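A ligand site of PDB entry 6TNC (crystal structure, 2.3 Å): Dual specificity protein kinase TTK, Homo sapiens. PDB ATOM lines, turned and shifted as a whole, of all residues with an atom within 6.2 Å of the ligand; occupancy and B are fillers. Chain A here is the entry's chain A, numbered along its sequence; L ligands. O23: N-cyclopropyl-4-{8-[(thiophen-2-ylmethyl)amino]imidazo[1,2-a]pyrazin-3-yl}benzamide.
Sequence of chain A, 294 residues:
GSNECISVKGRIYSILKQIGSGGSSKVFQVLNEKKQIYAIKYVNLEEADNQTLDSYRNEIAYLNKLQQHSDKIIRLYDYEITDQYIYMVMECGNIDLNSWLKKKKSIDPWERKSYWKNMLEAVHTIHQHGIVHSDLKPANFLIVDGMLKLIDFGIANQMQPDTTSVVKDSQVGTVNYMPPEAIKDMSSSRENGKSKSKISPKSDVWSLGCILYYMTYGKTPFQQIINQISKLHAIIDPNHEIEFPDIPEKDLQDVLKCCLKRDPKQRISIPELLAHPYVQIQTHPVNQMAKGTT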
ATOM      1  N   LYS A  17     -10.443   6.166 -26.452  1.00  0.00           N
ATOM      2  CA  LYS A  17     -11.364   5.659 -27.462  1.00  0.00           C
ATOM      3  C   LYS A  17     -12.323   4.619 -26.875  1.00  0.00           C
ATOM      4  O   LYS A  17     -12.106   4.091 -25.792  1.00  0.00           O
ATOM      5  CB  LYS A  17     -10.618   5.063 -28.670  1.00  0.00           C
ATOM      6  CG  LYS A  17      -9.619   3.956 -28.344  1.00  0.00           C
ATOM      7  CD  LYS A  17      -8.945   3.417 -29.607  1.00  0.00           C
ATOM      8  CE  LYS A  17      -7.777   4.281 -30.101  1.00  0.00           C
ATOM      9  NZ  LYS A  17      -6.470   3.903 -29.495  1.00  0.00           N
ATOM     10  N   GLN A  18     -13.368   4.357 -27.641  1.00  0.00           N
ATOM     11  CA  GLN A  18     -14.377   3.377 -27.315  1.00  0.00           C
ATOM     12  C   GLN A  18     -13.944   2.010 -27.823  1.00  0.00           C
ATOM     13  O   GLN A  18     -13.876   1.791 -29.025  1.00  0.00           O
ATOM     14  CB  GLN A  18     -15.709   3.784 -27.938  1.00  0.00           C
ATOM     15  CG  GLN A  18     -16.835   2.797 -27.640  1.00  0.00           C
ATOM     16  CD  GLN A  18     -18.205   3.419 -27.424  1.00  0.00           C
ATOM     17  OE1 GLN A  18     -18.328   4.614 -27.176  1.00  0.00           O
ATOM     18  NE2 GLN A  18     -19.231   2.598 -27.515  1.00  0.00           N
ATOM     19  N   ILE A  19     -13.688   1.086 -26.903  1.00  0.00           N
ATOM     20  CA  ILE A  19     -13.264  -0.265 -27.244  1.00  0.00           C
ATOM     21  C   ILE A  19     -14.453  -1.101 -27.695  1.00  0.00           C
ATOM     22  O   ILE A  19     -14.377  -1.787 -28.710  1.00  0.00           O
ATOM     23  CB  ILE A  19     -12.620  -0.962 -26.038  1.00  0.00           C
ATOM     24  CG1 ILE A  19     -11.359  -0.220 -25.585  1.00  0.00           C
ATOM     25  CG2 ILE A  19     -12.286  -2.418 -26.371  1.00  0.00           C
ATOM     26  CD1 ILE A  19     -10.811  -0.653 -24.237  1.00  0.00           C
ATOM     27  N   VAL A  27     -17.331   0.191 -23.129  1.00  0.00           N
ATOM     28  CA  VAL A  27     -15.998   0.019 -22.591  1.00  0.00           C
ATOM     29  C   VAL A  27     -15.091   1.034 -23.273  1.00  0.00           C
ATOM     30  O   VAL A  27     -15.121   1.152 -24.480  1.00  0.00           O
ATOM     31  CB  VAL A  27     -15.474  -1.397 -22.832  1.00  0.00           C
ATOM     32  CG1 VAL A  27     -14.164  -1.593 -22.080  1.00  0.00           C
ATOM     33  CG2 VAL A  27     -16.502  -2.438 -22.397  1.00  0.00           C
ATOM     34  N   GLN A  29     -11.128   2.750 -23.514  1.00  0.00           N
ATOM     35  CA  GLN A  29      -9.723   2.855 -23.176  1.00  0.00           C
ATOM     36  C   GLN A  29      -9.553   4.253 -22.617  1.00  0.00           C
ATOM     37  O   GLN A  29     -10.029   5.240 -23.207  1.00  0.00           O
ATOM     38  CB  GLN A  29      -8.840   2.657 -24.400  1.00  0.00           C
ATOM     39  CG  GLN A  29      -7.354   2.653 -24.074  1.00  0.00           C
ATOM     40  CD  GLN A  29      -6.503   2.722 -25.330  1.00  0.00           C
ATOM     41  OE1 GLN A  29      -6.871   3.344 -26.307  1.00  0.00           O
ATOM     42  NE2 GLN A  29      -5.357   2.055 -25.295  1.00  0.00           N
ATOM     43  N   ALA A  39      -8.913   0.185 -18.965  1.00  0.00           N
ATOM     44  CA  ALA A  39     -10.164   0.016 -19.650  1.00  0.00           C
ATOM     45  C   ALA A  39     -11.248   0.159 -18.606  1.00  0.00           C
ATOM     46  O   ALA A  39     -11.190  -0.496 -17.561  1.00  0.00           O
ATOM     47  CB  ALA A  39     -10.228  -1.342 -20.335  1.00  0.00           C
ATOM     48  N   LYS A  41     -15.332  -0.097 -18.009  1.00  0.00           N
ATOM     49  CA  LYS A  41     -16.648  -0.486 -18.465  1.00  0.00           C
ATOM     50  C   LYS A  41     -17.659   0.344 -17.708  1.00  0.00           C
ATOM     51  O   LYS A  41     -17.550   0.480 -16.482  1.00  0.00           O
ATOM     52  CB  LYS A  41     -16.870  -1.948 -18.168  1.00  0.00           C
ATOM     53  CG  LYS A  41     -18.145  -2.533 -18.772  1.00  0.00           C
ATOM     54  CD  LYS A  41     -18.291  -3.946 -18.251  1.00  0.00           C
ATOM     55  CE  LYS A  41     -19.299  -4.740 -19.011  1.00  0.00           C
ATOM     56  NZ  LYS A  41     -19.216  -6.128 -18.499  1.00  0.00           N
ATOM     57  N   GLU A  59     -21.783 -10.741 -12.267  1.00  0.00           N
ATOM     58  CA  GLU A  59     -20.536 -10.590 -12.996  1.00  0.00           C
ATOM     59  C   GLU A  59     -19.463  -9.899 -12.139  1.00  0.00           C
ATOM     60  O   GLU A  59     -18.310 -10.364 -12.080  1.00  0.00           O
ATOM     61  CB  GLU A  59     -20.778  -9.771 -14.301  1.00  0.00           C
ATOM     62  CG  GLU A  59     -19.550  -9.641 -15.188  1.00  0.00           C
ATOM     63  CD  GLU A  59     -19.813  -8.893 -16.494  1.00  0.00           C
ATOM     64  OE1 GLU A  59     -20.016  -7.643 -16.498  1.00  0.00           O
ATOM     65  OE2 GLU A  59     -19.770  -9.568 -17.540  1.00  0.00           O
ATOM     66  N   LEU A  63     -16.075 -11.556 -10.944  1.00  0.00           N
ATOM     67  CA  LEU A  63     -14.824 -10.906 -11.332  1.00  0.00           C
ATOM     68  C   LEU A  63     -13.963 -10.553 -10.092  1.00  0.00           C
ATOM     69  O   LEU A  63     -12.754 -10.760 -10.102  1.00  0.00           O
ATOM     70  CB  LEU A  63     -15.097  -9.659 -12.173  1.00  0.00           C
ATOM     71  CG  LEU A  63     -13.884  -8.901 -12.706  1.00  0.00           C
ATOM     72  CD1 LEU A  63     -12.970  -9.791 -13.527  1.00  0.00           C
ATOM     73  CD2 LEU A  63     -14.312  -7.664 -13.495  1.00  0.00           C
ATOM     74  N   ILE A  74      -8.931 -11.334 -16.341  1.00  0.00           N
ATOM     75  CA  ILE A  74      -8.711  -9.884 -16.431  1.00  0.00           C
ATOM     76  C   ILE A  74      -8.657  -9.195 -15.041  1.00  0.00           C
ATOM     77  O   ILE A  74      -9.458  -9.483 -14.148  1.00  0.00           O
ATOM     78  CB  ILE A  74      -9.777  -9.238 -17.343  1.00  0.00           C
ATOM     79  CG1 ILE A  74      -9.365  -7.838 -17.784  1.00  0.00           C
ATOM     80  CG2 ILE A  74     -11.156  -9.246 -16.689  1.00  0.00           C
ATOM     81  CD1 ILE A  74      -8.407  -7.851 -18.954  1.00  0.00           C
ATOM     82  N   MET A  88     -16.497  -0.341 -13.908  1.00  0.00           N
ATOM     83  CA  MET A  88     -15.454  -1.291 -13.573  1.00  0.00           C
ATOM     84  C   MET A  88     -14.158  -0.790 -14.228  1.00  0.00           C
ATOM     85  O   MET A  88     -14.117  -0.595 -15.459  1.00  0.00           O
ATOM     86  CB  MET A  88     -15.810  -2.668 -14.118  1.00  0.00           C
ATOM     87  CG  MET A  88     -17.152  -3.207 -13.648  1.00  0.00           C
ATOM     88  SD  MET A  88     -17.553  -4.800 -14.399  1.00  0.00           S
ATOM     89  CE  MET A  88     -19.310  -4.604 -14.576  1.00  0.00           C
ATOM     90  N   MET A  90     -10.639  -1.751 -15.179  1.00  0.00           N
ATOM     91  CA  MET A  90      -9.950  -2.981 -15.482  1.00  0.00           C
ATOM     92  C   MET A  90      -8.695  -2.678 -16.276  1.00  0.00           C
ATOM     93  O   MET A  90      -8.496  -1.534 -16.715  1.00  0.00           O
ATOM     94  CB  MET A  90     -10.862  -3.875 -16.305  1.00  0.00           C
ATOM     95  CG  MET A  90     -12.141  -4.243 -15.563  1.00  0.00           C
ATOM     96  SD  MET A  90     -13.298  -5.209 -16.532  1.00  0.00           S
ATOM     97  CE  MET A  90     -13.778  -4.023 -17.776  1.00  0.00           C
ATOM     98  N   GLU A  91      -7.838  -3.689 -16.422  1.00  0.00           N
ATOM     99  CA  GLU A  91      -6.594  -3.527 -17.178  1.00  0.00           C
ATOM    100  C   GLU A  91      -6.959  -3.432 -18.644  1.00  0.00           C
ATOM    101  O   GLU A  91      -7.982  -3.985 -19.098  1.00  0.00           O
ATOM    102  CB  GLU A  91      -5.573  -4.669 -16.921  1.00  0.00           C
ATOM    103  CG  GLU A  91      -5.940  -6.030 -17.489  1.00  0.00           C
ATOM    104  CD  GLU A  91      -4.995  -7.149 -17.070  1.00  0.00           C
ATOM    105  OE1 GLU A  91      -3.751  -7.008 -17.095  1.00  0.00           O
ATOM    106  OE2 GLU A  91      -5.525  -8.213 -16.708  1.00  0.00           O
ATOM    107  N   CYS A  92      -6.137  -2.706 -19.381  1.00  0.00           N
ATOM    108  CA  CYS A  92      -6.306  -2.576 -20.796  1.00  0.00           C
ATOM    109  C   CYS A  92      -5.362  -3.507 -21.500  1.00  0.00           C
ATOM    110  O   CYS A  92      -4.145  -3.424 -21.286  1.00  0.00           O
ATOM    111  CB  CYS A  92      -6.059  -1.126 -21.261  1.00  0.00           C
ATOM    112  SG  CYS A  92      -6.688  -0.900 -22.945  1.00  0.00           S
ATOM    113  N   GLY A  93      -5.895  -4.364 -22.367  1.00  0.00           N
ATOM    114  CA  GLY A  93      -5.063  -5.298 -23.128  1.00  0.00           C
ATOM    115  C   GLY A  93      -4.382  -4.681 -24.339  1.00  0.00           C
ATOM    116  O   GLY A  93      -4.725  -3.597 -24.763  1.00  0.00           O
ATOM    117  N   ASN A  94      -3.427  -5.414 -24.908  1.00  0.00           N
ATOM    118  CA  ASN A  94      -2.772  -5.018 -26.148  1.00  0.00           C
ATOM    119  C   ASN A  94      -3.728  -5.183 -27.313  1.00  0.00           C
ATOM    120  O   ASN A  94      -3.921  -4.255 -28.102  1.00  0.00           O
ATOM    121  CB  ASN A  94      -1.515  -5.870 -26.377  1.00  0.00           C
ATOM    122  CG  ASN A  94      -0.442  -5.605 -25.339  1.00  0.00           C
ATOM    123  OD1 ASN A  94      -0.658  -5.790 -24.138  1.00  0.00           O
ATOM    124  ND2 ASN A  94       0.727  -5.173 -25.793  1.00  0.00           N
ATOM    125  N   ILE A  95      -4.327  -6.362 -27.412  1.00  0.00           N
ATOM    126  CA  ILE A  95      -5.210  -6.729 -28.518  1.00  0.00           C
ATOM    127  C   ILE A  95      -5.963  -7.996 -28.124  1.00  0.00           C
ATOM    128  O   ILE A  95      -5.456  -8.784 -27.325  1.00  0.00           O
ATOM    129  CB  ILE A  95      -4.394  -6.960 -29.823  1.00  0.00           C
ATOM    130  CG1 ILE A  95      -5.312  -7.204 -31.030  1.00  0.00           C
ATOM    131  CG2 ILE A  95      -3.410  -8.110 -29.664  1.00  0.00           C
ATOM    132  CD1 ILE A  95      -4.555  -7.092 -32.359  1.00  0.00           C
ATOM    133  N   ASP A  96      -7.161  -8.171 -28.680  1.00  0.00           N
ATOM    134  CA  ASP A  96      -7.983  -9.355 -28.415  1.00  0.00           C
ATOM    135  C   ASP A  96      -7.617 -10.469 -29.382  1.00  0.00           C
ATOM    136  O   ASP A  96      -7.139 -10.199 -30.482  1.00  0.00           O
ATOM    137  CB  ASP A  96      -9.480  -9.017 -28.453  1.00  0.00           C
ATOM    138  CG  ASP A  96      -9.983  -8.758 -29.857  1.00  0.00           C
ATOM    139  OD1 ASP A  96     -10.404  -9.721 -30.519  1.00  0.00           O
ATOM    140  OD2 ASP A  96      -9.966  -7.586 -30.288  1.00  0.00           O
ATOM    141  N   ALA A 139     -12.812 -13.647 -29.422  1.00  0.00           N
ATOM    142  CA  ALA A 139     -13.079 -12.327 -28.829  1.00  0.00           C
ATOM    143  C   ALA A 139     -13.157 -12.293 -27.285  1.00  0.00           C
ATOM    144  O   ALA A 139     -12.921 -11.239 -26.683  1.00  0.00           O
ATOM    145  CB  ALA A 139     -14.357 -11.744 -29.430  1.00  0.00           C
ATOM    146  N   LEU A 142      -7.906 -12.030 -24.436  1.00  0.00           N
ATOM    147  CA  LEU A 142      -7.234 -10.791 -24.610  1.00  0.00           C
ATOM    148  C   LEU A 142      -5.767 -11.034 -24.388  1.00  0.00           C
ATOM    149  O   LEU A 142      -5.412 -11.749 -23.476  1.00  0.00           O
ATOM    150  CB  LEU A 142      -7.784  -9.802 -23.586  1.00  0.00           C
ATOM    151  CG  LEU A 142      -7.248  -8.363 -23.608  1.00  0.00           C
ATOM    152  CD1 LEU A 142      -7.768  -7.613 -24.832  1.00  0.00           C
ATOM    153  CD2 LEU A 142      -7.642  -7.631 -22.327  1.00  0.00           C
ATOM    154  N   ILE A 151     -11.623 -12.539 -20.522  1.00  0.00           N
ATOM    155  CA  ILE A 151     -12.127 -11.217 -20.114  1.00  0.00           C
ATOM    156  C   ILE A 151     -13.518 -11.207 -19.521  1.00  0.00           C
ATOM    157  O   ILE A 151     -13.855 -10.231 -18.875  1.00  0.00           O
ATOM    158  CB  ILE A 151     -12.056 -10.139 -21.241  1.00  0.00           C
ATOM    159  CG1 ILE A 151     -13.112 -10.378 -22.324  1.00  0.00           C
ATOM    160  CG2 ILE A 151     -10.649 -10.082 -21.804  1.00  0.00           C
ATOM    161  CD1 ILE A 151     -12.925  -9.511 -23.559  1.00  0.00           C
ATOM    162  N   ASP A 152     -14.305 -12.245 -19.782  1.00  0.00           N
ATOM    163  CA  ASP A 152     -15.655 -12.331 -19.252  1.00  0.00           C
ATOM    164  C   ASP A 152     -16.080 -13.786 -19.012  1.00  0.00           C
ATOM    165  O   ASP A 152     -15.353 -14.712 -19.332  1.00  0.00           O
ATOM    166  CB  ASP A 152     -16.611 -11.657 -20.227  1.00  0.00           C
ATOM    167  CG  ASP A 152     -16.803 -12.457 -21.483  1.00  0.00           C
ATOM    168  OD1 ASP A 152     -15.823 -13.085 -21.924  1.00  0.00           O
ATOM    169  OD2 ASP A 152     -17.935 -12.490 -22.016  1.00  0.00           O
ATOM    170  N   PHE A 153     -17.275 -13.962 -18.466  1.00  0.00           N
ATOM    171  CA  PHE A 153     -17.674 -15.262 -17.911  1.00  0.00           C
ATOM    172  C   PHE A 153     -18.949 -15.788 -18.508  1.00  0.00           C
ATOM    173  O   PHE A 153     -19.484 -16.752 -18.009  1.00  0.00           O
ATOM    174  CB  PHE A 153     -17.860 -15.138 -16.406  1.00  0.00           C
ATOM    175  CG  PHE A 153     -16.766 -14.406 -15.740  1.00  0.00           C
ATOM    176  CD1 PHE A 153     -15.464 -14.826 -15.879  1.00  0.00           C
ATOM    177  CD2 PHE A 153     -17.048 -13.278 -14.990  1.00  0.00           C
ATOM    178  CE1 PHE A 153     -14.430 -14.130 -15.274  1.00  0.00           C
ATOM    179  CE2 PHE A 153     -16.015 -12.574 -14.374  1.00  0.00           C
ATOM    180  CZ  PHE A 153     -14.703 -13.014 -14.514  1.00  0.00           C
ATOM    181  N   MET A 159     -19.409  -7.987 -24.868  1.00  0.00           N
ATOM    182  CA  MET A 159     -18.942  -6.822 -25.633  1.00  0.00           C
ATOM    183  C   MET A 159     -18.905  -7.088 -27.153  1.00  0.00           C
ATOM    184  O   MET A 159     -18.477  -8.160 -27.595  1.00  0.00           O
ATOM    185  CB  MET A 159     -17.551  -6.444 -25.113  1.00  0.00           C
ATOM    186  CG  MET A 159     -16.854  -5.268 -25.794  1.00  0.00           C
ATOM    187  SD  MET A 159     -15.059  -5.281 -25.612  1.00  0.00           S
ATOM    188  CE  MET A 159     -14.600  -6.885 -26.282  1.00  0.00           C
HETATM  189  O   O23 L   1     -16.496  -6.330 -19.840  1.00  0.00           O
HETATM  190  C   O23 L   1     -15.446  -6.941 -19.688  1.00  0.00           C
HETATM  191  N   O23 L   1     -15.322  -7.994 -18.901  1.00  0.00           N
HETATM  192  C1  O23 L   1     -16.457  -8.508 -18.117  1.00  0.00           C
HETATM  193  C3  O23 L   1     -16.080  -9.145 -16.774  1.00  0.00           C
HETATM  194  C2  O23 L   1     -16.695  -7.733 -16.822  1.00  0.00           C
HETATM  195  C4  O23 L   1     -14.193  -6.476 -20.428  1.00  0.00           C
HETATM  196  C9  O23 L   1     -12.929  -6.560 -19.841  1.00  0.00           C
HETATM  197  C8  O23 L   1     -11.789  -6.136 -20.500  1.00  0.00           C
HETATM  198  C7  O23 L   1     -11.902  -5.595 -21.788  1.00  0.00           C
HETATM  199  C6  O23 L   1     -13.164  -5.495 -22.369  1.00  0.00           C
HETATM  200  C5  O23 L   1     -14.308  -5.927 -21.705  1.00  0.00           C
HETATM  201  C10 O23 L   1     -10.751  -5.140 -22.452  1.00  0.00           C
HETATM  202  N2  O23 L   1     -10.574  -5.174 -23.839  1.00  0.00           N
HETATM  203  C13 O23 L   1     -11.350  -5.625 -24.920  1.00  0.00           C
HETATM  204  C14 O23 L   1     -10.836  -5.501 -26.216  1.00  0.00           C
HETATM  205  N3  O23 L   1      -9.631  -4.971 -26.408  1.00  0.00           N
HETATM  206  C15 O23 L   1      -8.861  -4.525 -25.397  1.00  0.00           C
HETATM  207  C12 O23 L   1      -9.319  -4.631 -24.070  1.00  0.00           C
HETATM  208  N1  O23 L   1      -8.789  -4.284 -22.894  1.00  0.00           N
HETATM  209  C11 O23 L   1      -9.654  -4.589 -21.924  1.00  0.00           C
HETATM  210  N4  O23 L   1      -7.662  -4.004 -25.645  1.00  0.00           N
HETATM  211  C16 O23 L   1      -7.202  -3.683 -27.013  1.00  0.00           C
HETATM  212  C17 O23 L   1      -7.799  -2.351 -27.519  1.00  0.00           C
HETATM  213  S   O23 L   1      -7.243  -0.837 -27.020  1.00  0.00           S
HETATM  214  C20 O23 L   1      -8.333   0.039 -27.972  1.00  0.00           C
HETATM  215  C19 O23 L   1      -9.080  -0.861 -28.633  1.00  0.00           C
HETATM  216  C18 O23 L   1      -8.800  -2.160 -28.391  1.00  0.00           C
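The side-chain amino group (NZ) of Lys 41 lies within hydrogen-bond range of an oxygen (O) of the ligand, at 3.0 Å. N of Gly 93 sits at hydrogen-bond distance from N1 of the ligand (2.9 Å). O of Ile 151 lies within hydrogen-bond range of N of the ligand (2.7 Å). O of Gly 93 lies within hydrogen-bond range of N4 of the ligand.
Merely in contact with the ligand: Leu 142 (3.3 Å), Glu 59 (3.3 Å), Glu 91 (3.3 Å), Met 90 (3.4 Å), Ile 19 (3.4 Å), Asn 94 (3.5 Å), Ala 39 (3.7 Å), Cys 92 (3.7 Å), Met 159 (3.7 Å), Asp 152 (3.8 Å), Lys 17 (3.8 Å), Gln 29 (3.9 Å), Met 88 (3.9 Å) and Ile 95 (3.9 Å). Hydrophobic or aromatic side chains within 4 Å of the ligand: Ile 19, Ala 39, Met 88, Met 90, Leu 142, Ile 151 and Met 159. 17 residues have an atom within 4 Å of the ligand: Lys 17, Ile 19, Gln 29, Ala 39, Lys 41, Glu 59, Met 88, Met 90, Glu 91, Cys 92, Gly 93, Asn 94, Ile 95, Leu 142, Ile 151, Asp 152 and Met 159. The nearest printed residue that does not touch the ligand is Leu 63 (4.01 Å).
The backbone NH of Lys 41 lies within hydrogen-bond range of the backbone carbonyl oxygen of Met 88 (2.9 Å). N of Gln 29 is in hydrogen-bond range of O of Lys 17 (2.8 Å). NZ of Lys 41 is in salt-bridge range of OE1 of Glu 59 (2.6 Å). The backbone NH (N) of Ile 19 sits at hydrogen-bond distance from the backbone carbonyl oxygen (O) of Val 27 (2.8 Å). The backbone NH (N) of Met 90 lies within hydrogen-bond range of the backbone carbonyl oxygen (O) of Ala 39 (2.7 Å).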
